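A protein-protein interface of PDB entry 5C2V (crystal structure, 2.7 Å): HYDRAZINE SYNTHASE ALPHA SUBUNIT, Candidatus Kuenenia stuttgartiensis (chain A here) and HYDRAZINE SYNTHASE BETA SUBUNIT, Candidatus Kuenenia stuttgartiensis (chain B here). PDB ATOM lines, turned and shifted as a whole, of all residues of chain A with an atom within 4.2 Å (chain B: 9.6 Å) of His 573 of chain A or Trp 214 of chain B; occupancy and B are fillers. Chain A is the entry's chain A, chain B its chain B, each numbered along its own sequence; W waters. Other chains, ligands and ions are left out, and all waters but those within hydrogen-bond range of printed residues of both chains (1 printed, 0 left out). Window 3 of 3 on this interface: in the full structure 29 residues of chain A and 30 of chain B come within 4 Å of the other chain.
ND2 of Asn 571 of chain A is in hydrogen-bond range of OE2 of Glu 188 of chain B, 3.4 Å away. The side-chain amide nitrogen (ND2) of Asn 571 of chain A lies within hydrogen-bond range of the side-chain amide oxygen (OD1) of Asn 213 of chain B (3.4 Å). The backbone NH (N) of Trp 214 of chain B sits at hydrogen-bond distance from the side-chain amide oxygen (OD1) of Asn 571 of chain A, 3.2 Å away. O of Ile 572 of chain A lies close to O of Trp 214 of chain B.
A ring nitrogen (NE2) of His 573 of chain A sits at hydrogen-bond distance from the side-chain hydroxyl of Tyr 578 of chain A, at 2.8 Å. The backbone carbonyl oxygen (O) of Glu 188 of chain B lies close to the side-chain hydroxyl (OG1) of Thr 210 of chain B, 3.5 Å away. The backbone NH of Lys 212 of chain B lies within hydrogen-bond range of the backbone carbonyl oxygen of Val 225 of chain B, at 2.8 Å. The indole nitrogen of Trp 214 of chain B lies close to the side-chain amide nitrogen of Asn 213 of chain B, 3.0 Å away.
CA of Lys 212 of chain B touches OD1 of Asn 571 of chain A (3.6 Å). Leu 215 of chain B touches Ile 572 of chain A. CZ3 of Trp 214 of chain B touches CE1 of His 573 of chain A, at 3.4 Å. CD2 of Leu 577 of chain A touches O of Trp 214 of chain B (3.97 Å). Pro 216 of chain B touches Leu 577 of chain A (CG to CD1, 3.6 Å).
His 573 of chain A touches just one residue of chain B: Trp 214 (3.4 Å). Asn 167 of chain B touches none of the printed residues of chain A. Of the printed residues of chain A, Lys 212 of chain B touches Asn 571. Trp 214 of chain B touches just these residues of chain A: Asn 571, Ile 572, His 573 and Leu 577. Of the printed residues of chain A, Pro 216 of chain B touches Leu 577. The nearest residue of chain B that does not touch His 573 of chain A is Leu 215 of chain B (5.5 Å).
Hydrophobic or aromatic side chains of chain B within 4 Å of the printed part of chain A: Trp 214, Leu 215 and Pro 216. Among the printed residues, 9 pairs touch across the chains. Among the printed residues, no Asp or Glu carboxylate lies within 4 Å of a Lys or Arg side-chain nitrogen of the other chain.
Water W1 lies within hydrogen-bond range of the backbone NH (N) of Ala 574 of chain A (2.7 Å), the backbone carbonyl oxygen (O) of Ile 572 of chain A (2.8 Å) and the backbone carbonyl oxygen (O) of Trp 214 of chain B (3.0 Å).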
ATOM      1  N   ASP A 514       6.788 -19.596 -19.076  1.00  0.00           N
ATOM      2  CA  ASP A 514       7.161 -19.432 -17.674  1.00  0.00           C
ATOM      3  C   ASP A 514       6.178 -18.514 -16.948  1.00  0.00           C
ATOM      4  O   ASP A 514       6.352 -18.213 -15.768  1.00  0.00           O
ATOM      5  CB  ASP A 514       8.590 -18.893 -17.552  1.00  0.00           C
ATOM      6  CG  ASP A 514       8.741 -17.492 -18.113  1.00  0.00           C
ATOM      7  OD1 ASP A 514       7.894 -17.078 -18.930  1.00  0.00           O
ATOM      8  OD2 ASP A 514       9.715 -16.806 -17.738  1.00  0.00           O
ATOM      9  N   ASN A 571      12.752 -12.893  -6.794  1.00  0.00           N
ATOM     10  CA  ASN A 571      13.808 -12.965  -7.788  1.00  0.00           C
ATOM     11  C   ASN A 571      13.398 -13.967  -8.851  1.00  0.00           C
ATOM     12  O   ASN A 571      13.252 -15.160  -8.581  1.00  0.00           O
ATOM     13  CB  ASN A 571      15.140 -13.362  -7.148  1.00  0.00           C
ATOM     14  CG  ASN A 571      16.329 -13.072  -8.045  1.00  0.00           C
ATOM     15  OD1 ASN A 571      16.285 -12.169  -8.881  1.00  0.00           O
ATOM     16  ND2 ASN A 571      17.401 -13.837  -7.873  1.00  0.00           N
ATOM     17  N   ILE A 572      13.222 -13.468 -10.069  1.00  0.00           N
ATOM     18  CA  ILE A 572      12.698 -14.268 -11.165  1.00  0.00           C
ATOM     19  C   ILE A 572      13.458 -13.953 -12.440  1.00  0.00           C
ATOM     20  O   ILE A 572      13.643 -12.789 -12.793  1.00  0.00           O
ATOM     21  CB  ILE A 572      11.188 -14.011 -11.406  1.00  0.00           C
ATOM     22  CG1 ILE A 572      10.372 -14.264 -10.134  1.00  0.00           C
ATOM     23  CG2 ILE A 572      10.668 -14.878 -12.544  1.00  0.00           C
ATOM     24  CD1 ILE A 572       8.882 -14.069 -10.317  1.00  0.00           C
ATOM     25  N   HIS A 573      13.894 -14.996 -13.132  1.00  0.00           N
ATOM     26  CA  HIS A 573      14.544 -14.822 -14.416  1.00  0.00           C
ATOM     27  C   HIS A 573      13.512 -15.144 -15.486  1.00  0.00           C
ATOM     28  O   HIS A 573      13.164 -16.305 -15.699  1.00  0.00           O
ATOM     29  CB  HIS A 573      15.770 -15.729 -14.518  1.00  0.00           C
ATOM     30  CG  HIS A 573      16.696 -15.382 -15.640  1.00  0.00           C
ATOM     31  ND1 HIS A 573      17.852 -16.090 -15.891  1.00  0.00           N
ATOM     32  CD2 HIS A 573      16.645 -14.403 -16.573  1.00  0.00           C
ATOM     33  CE1 HIS A 573      18.470 -15.563 -16.933  1.00  0.00           C
ATOM     34  NE2 HIS A 573      17.759 -14.538 -17.365  1.00  0.00           N
ATOM     35  N   ALA A 574      13.030 -14.107 -16.164  1.00  0.00           N
ATOM     36  CA  ALA A 574      11.853 -14.243 -17.013  1.00  0.00           C
ATOM     37  C   ALA A 574      12.175 -14.058 -18.488  1.00  0.00           C
ATOM     38  O   ALA A 574      13.035 -13.256 -18.852  1.00  0.00           O
ATOM     39  CB  ALA A 574      10.784 -13.249 -16.582  1.00  0.00           C
ATOM     40  N   LEU A 577      11.599 -10.511 -20.117  1.00  0.00           N
ATOM     41  CA  LEU A 577      12.644  -9.512 -19.916  1.00  0.00           C
ATOM     42  C   LEU A 577      13.438  -9.256 -21.193  1.00  0.00           C
ATOM     43  O   LEU A 577      13.849  -8.128 -21.468  1.00  0.00           O
ATOM     44  CB  LEU A 577      13.590  -9.952 -18.796  1.00  0.00           C
ATOM     45  CG  LEU A 577      14.832  -9.085 -18.582  1.00  0.00           C
ATOM     46  CD1 LEU A 577      14.434  -7.664 -18.224  1.00  0.00           C
ATOM     47  CD2 LEU A 577      15.740  -9.679 -17.516  1.00  0.00           C
ATOM     48  N   TYR A 578      13.643 -10.309 -21.976  1.00  0.00           N
ATOM     49  CA  TYR A 578      14.427 -10.213 -23.198  1.00  0.00           C
ATOM     50  C   TYR A 578      13.569  -9.780 -24.384  1.00  0.00           C
ATOM     51  O   TYR A 578      14.087  -9.484 -25.459  1.00  0.00           O
ATOM     52  CB  TYR A 578      15.111 -11.549 -23.491  1.00  0.00           C
ATOM     53  CG  TYR A 578      16.093 -11.962 -22.417  1.00  0.00           C
ATOM     54  CD1 TYR A 578      17.418 -11.551 -22.468  1.00  0.00           C
ATOM     55  CD2 TYR A 578      15.692 -12.753 -21.347  1.00  0.00           C
ATOM     56  CE1 TYR A 578      18.320 -11.921 -21.486  1.00  0.00           C
ATOM     57  CE2 TYR A 578      16.587 -13.128 -20.361  1.00  0.00           C
ATOM     58  CZ  TYR A 578      17.899 -12.708 -20.436  1.00  0.00           C
ATOM     59  OH  TYR A 578      18.793 -13.078 -19.457  1.00  0.00           O
ATOM     60  N   GLY B 164      31.382 -12.312  -6.838  1.00  0.00           N
ATOM     61  CA  GLY B 164      30.804 -12.884  -8.040  1.00  0.00           C
ATOM     62  C   GLY B 164      29.915 -14.082  -7.772  1.00  0.00           C
ATOM     63  O   GLY B 164      29.689 -14.902  -8.662  1.00  0.00           O
ATOM     64  N   SER B 165      29.406 -14.185  -6.549  1.00  0.00           N
ATOM     65  CA  SER B 165      28.556 -15.312  -6.182  1.00  0.00           C
ATOM     66  C   SER B 165      27.211 -14.875  -5.610  1.00  0.00           C
ATOM     67  O   SER B 165      27.145 -14.043  -4.704  1.00  0.00           O
ATOM     68  CB  SER B 165      29.270 -16.212  -5.173  1.00  0.00           C
ATOM     69  OG  SER B 165      28.442 -17.297  -4.794  1.00  0.00           O
ATOM     70  N   ILE B 166      26.141 -15.440  -6.161  1.00  0.00           N
ATOM     71  CA  ILE B 166      24.801 -15.245  -5.624  1.00  0.00           C
ATOM     72  C   ILE B 166      24.582 -16.138  -4.412  1.00  0.00           C
ATOM     73  O   ILE B 166      23.991 -15.719  -3.416  1.00  0.00           O
ATOM     74  CB  ILE B 166      23.726 -15.545  -6.676  1.00  0.00           C
ATOM     75  CG1 ILE B 166      23.810 -14.524  -7.806  1.00  0.00           C
ATOM     76  CG2 ILE B 166      22.339 -15.520  -6.054  1.00  0.00           C
ATOM     77  CD1 ILE B 166      22.865 -14.811  -8.922  1.00  0.00           C
ATOM     78  N   ASN B 167      25.086 -17.363  -4.488  1.00  0.00           N
ATOM     79  CA  ASN B 167      24.946 -18.278  -3.373  1.00  0.00           C
ATOM     80  C   ASN B 167      26.238 -18.289  -2.576  1.00  0.00           C
ATOM     81  O   ASN B 167      27.261 -18.808  -3.021  1.00  0.00           O
ATOM     82  CB  ASN B 167      24.600 -19.686  -3.863  1.00  0.00           C
ATOM     83  CG  ASN B 167      23.610 -19.676  -5.011  1.00  0.00           C
ATOM     84  OD1 ASN B 167      22.396 -19.694  -4.803  1.00  0.00           O
ATOM     85  ND2 ASN B 167      24.126 -19.654  -6.233  1.00  0.00           N
ATOM     86  N   GLU B 188      20.716 -16.796  -2.472  1.00  0.00           N
ATOM     87  CA  GLU B 188      20.456 -15.398  -2.805  1.00  0.00           C
ATOM     88  C   GLU B 188      20.977 -14.444  -1.734  1.00  0.00           C
ATOM     89  O   GLU B 188      20.238 -13.601  -1.228  1.00  0.00           O
ATOM     90  CB  GLU B 188      18.959 -15.176  -3.031  1.00  0.00           C
ATOM     91  CG  GLU B 188      18.401 -15.955  -4.210  1.00  0.00           C
ATOM     92  CD  GLU B 188      16.979 -15.561  -4.551  1.00  0.00           C
ATOM     93  OE1 GLU B 188      16.393 -14.743  -3.811  1.00  0.00           O
ATOM     94  OE2 GLU B 188      16.446 -16.068  -5.562  1.00  0.00           O
ATOM     95  N   THR B 210      20.075  -9.538   0.520  1.00  0.00           N
ATOM     96  CA  THR B 210      19.500 -10.312  -0.566  1.00  0.00           C
ATOM     97  C   THR B 210      19.279  -9.419  -1.777  1.00  0.00           C
ATOM     98  O   THR B 210      18.375  -8.581  -1.784  1.00  0.00           O
ATOM     99  CB  THR B 210      18.160 -10.954  -0.156  1.00  0.00           C
ATOM    100  OG1 THR B 210      18.346 -11.761   1.014  1.00  0.00           O
ATOM    101  CG2 THR B 210      17.600 -11.807  -1.286  1.00  0.00           C
ATOM    102  N   PRO B 211      20.118  -9.589  -2.806  1.00  0.00           N
ATOM    103  CA  PRO B 211      19.926  -8.905  -4.083  1.00  0.00           C
ATOM    104  C   PRO B 211      18.839  -9.581  -4.899  1.00  0.00           C
ATOM    105  O   PRO B 211      18.701 -10.800  -4.800  1.00  0.00           O
ATOM    106  CB  PRO B 211      21.293  -9.044  -4.774  1.00  0.00           C
ATOM    107  CG  PRO B 211      22.095 -10.032  -3.935  1.00  0.00           C
ATOM    108  CD  PRO B 211      21.191 -10.594  -2.884  1.00  0.00           C
ATOM    109  N   LYS B 212      18.076  -8.837  -5.691  1.00  0.00           N
ATOM    110  CA  LYS B 212      17.419  -9.512  -6.791  1.00  0.00           C
ATOM    111  C   LYS B 212      18.223  -9.096  -8.012  1.00  0.00           C
ATOM    112  O   LYS B 212      18.091  -7.980  -8.514  1.00  0.00           O
ATOM    113  CB  LYS B 212      15.948  -9.107  -6.902  1.00  0.00           C
ATOM    114  CG  LYS B 212      15.332  -8.614  -5.591  1.00  0.00           C
ATOM    115  CD  LYS B 212      15.088  -9.731  -4.591  1.00  0.00           C
ATOM    116  CE  LYS B 212      14.506  -9.182  -3.294  1.00  0.00           C
ATOM    117  NZ  LYS B 212      14.076 -10.265  -2.366  1.00  0.00           N
ATOM    118  N   ASN B 213      19.056 -10.017  -8.482  1.00  0.00           N
ATOM    119  CA  ASN B 213      19.960  -9.766  -9.598  1.00  0.00           C
ATOM    120  C   ASN B 213      19.327  -9.977 -10.966  1.00  0.00           C
ATOM    121  O   ASN B 213      19.709  -9.341 -11.948  1.00  0.00           O
ATOM    122  CB  ASN B 213      21.207 -10.634  -9.450  1.00  0.00           C
ATOM    123  CG  ASN B 213      20.883 -12.102  -9.388  1.00  0.00           C
ATOM    124  OD1 ASN B 213      20.538 -12.633  -8.332  1.00  0.00           O
ATOM    125  ND2 ASN B 213      20.999 -12.773 -10.523  1.00  0.00           N
ATOM    126  N   TRP B 214      18.358 -10.885 -11.015  1.00  0.00           N
ATOM    127  CA  TRP B 214      17.748 -11.321 -12.266  1.00  0.00           C
ATOM    128  C   TRP B 214      16.616 -10.392 -12.682  1.00  0.00           C
ATOM    129  O   TRP B 214      15.927 -10.642 -13.671  1.00  0.00           O
ATOM    130  CB  TRP B 214      17.237 -12.760 -12.153  1.00  0.00           C
ATOM    131  CG  TRP B 214      18.325 -13.775 -11.949  1.00  0.00           C
ATOM    132  CD1 TRP B 214      18.539 -14.535 -10.836  1.00  0.00           C
ATOM    133  CD2 TRP B 214      19.356 -14.130 -12.879  1.00  0.00           C
ATOM    134  NE1 TRP B 214      19.631 -15.350 -11.020  1.00  0.00           N
ATOM    135  CE2 TRP B 214      20.151 -15.118 -12.265  1.00  0.00           C
ATOM    136  CE3 TRP B 214      19.681 -13.711 -14.173  1.00  0.00           C
ATOM    137  CZ2 TRP B 214      21.252 -15.692 -12.900  1.00  0.00           C
ATOM    138  CZ3 TRP B 214      20.773 -14.281 -14.801  1.00  0.00           C
ATOM    139  CH2 TRP B 214      21.545 -15.261 -14.164  1.00  0.00           C
ATOM    140  N   LEU B 215      16.429  -9.319 -11.923  1.00  0.00           N
ATOM    141  CA  LEU B 215      15.330  -8.402 -12.171  1.00  0.00           C
ATOM    142  C   LEU B 215      15.862  -7.069 -12.670  1.00  0.00           C
ATOM    143  O   LEU B 215      16.979  -6.674 -12.334  1.00  0.00           O
ATOM    144  CB  LEU B 215      14.511  -8.182 -10.894  1.00  0.00           C
ATOM    145  CG  LEU B 215      13.669  -9.326 -10.329  1.00  0.00           C
ATOM    146  CD1 LEU B 215      12.894  -8.843  -9.113  1.00  0.00           C
ATOM    147  CD2 LEU B 215      12.726  -9.876 -11.385  1.00  0.00           C
ATOM    148  N   PRO B 216      15.056  -6.370 -13.483  1.00  0.00           N
ATOM    149  CA  PRO B 216      15.417  -5.045 -13.989  1.00  0.00           C
ATOM    150  C   PRO B 216      15.583  -4.063 -12.844  1.00  0.00           C
ATOM    151  O   PRO B 216      14.910  -4.209 -11.826  1.00  0.00           O
ATOM    152  CB  PRO B 216      14.220  -4.663 -14.866  1.00  0.00           C
ATOM    153  CG  PRO B 216      13.578  -5.952 -15.222  1.00  0.00           C
ATOM    154  CD  PRO B 216      13.778  -6.843 -14.041  1.00  0.00           C
ATOM    155  N   VAL B 217      16.458  -3.078 -12.998  1.00  0.00           N
ATOM    156  CA  VAL B 217      16.576  -2.067 -11.965  1.00  0.00           C
ATOM    157  C   VAL B 217      15.649  -0.931 -12.365  1.00  0.00           C
ATOM    158  O   VAL B 217      15.907  -0.202 -13.324  1.00  0.00           O
ATOM    159  CB  VAL B 217      18.027  -1.577 -11.804  1.00  0.00           C
ATOM    160  CG1 VAL B 217      18.154  -0.687 -10.584  1.00  0.00           C
ATOM    161  CG2 VAL B 217      18.965  -2.766 -11.682  1.00  0.00           C
ATOM    162  N   GLN B 224      13.029  -4.023  -4.322  1.00  0.00           N
ATOM    163  CA  GLN B 224      13.146  -4.582  -5.667  1.00  0.00           C
ATOM    164  C   GLN B 224      14.590  -4.910  -6.032  1.00  0.00           C
ATOM    165  O   GLN B 224      14.854  -5.845  -6.786  1.00  0.00           O
ATOM    166  CB  GLN B 224      12.564  -3.620  -6.707  1.00  0.00           C
ATOM    167  CG  GLN B 224      12.661  -4.151  -8.130  1.00  0.00           C
ATOM    168  CD  GLN B 224      12.792  -3.057  -9.164  1.00  0.00           C
ATOM    169  OE1 GLN B 224      12.307  -1.946  -8.972  1.00  0.00           O
ATOM    170  NE2 GLN B 224      13.462  -3.366 -10.266  1.00  0.00           N
ATOM    171  N   VAL B 225      15.523  -4.129  -5.503  1.00  0.00           N
ATOM    172  CA  VAL B 225      16.936  -4.336  -5.788  1.00  0.00           C
ATOM    173  C   VAL B 225      17.602  -5.081  -4.638  1.00  0.00           C
ATOM    174  O   VAL B 225      18.075  -6.205  -4.805  1.00  0.00           O
ATOM    175  CB  VAL B 225      17.663  -3.003  -6.039  1.00  0.00           C
ATOM    176  CG1 VAL B 225      19.134  -3.248  -6.331  1.00  0.00           C
ATOM    177  CG2 VAL B 225      17.004  -2.252  -7.188  1.00  0.00           C
HETATM  178  O   HOH W   1      13.688 -11.664 -15.350  1.00  0.00           O
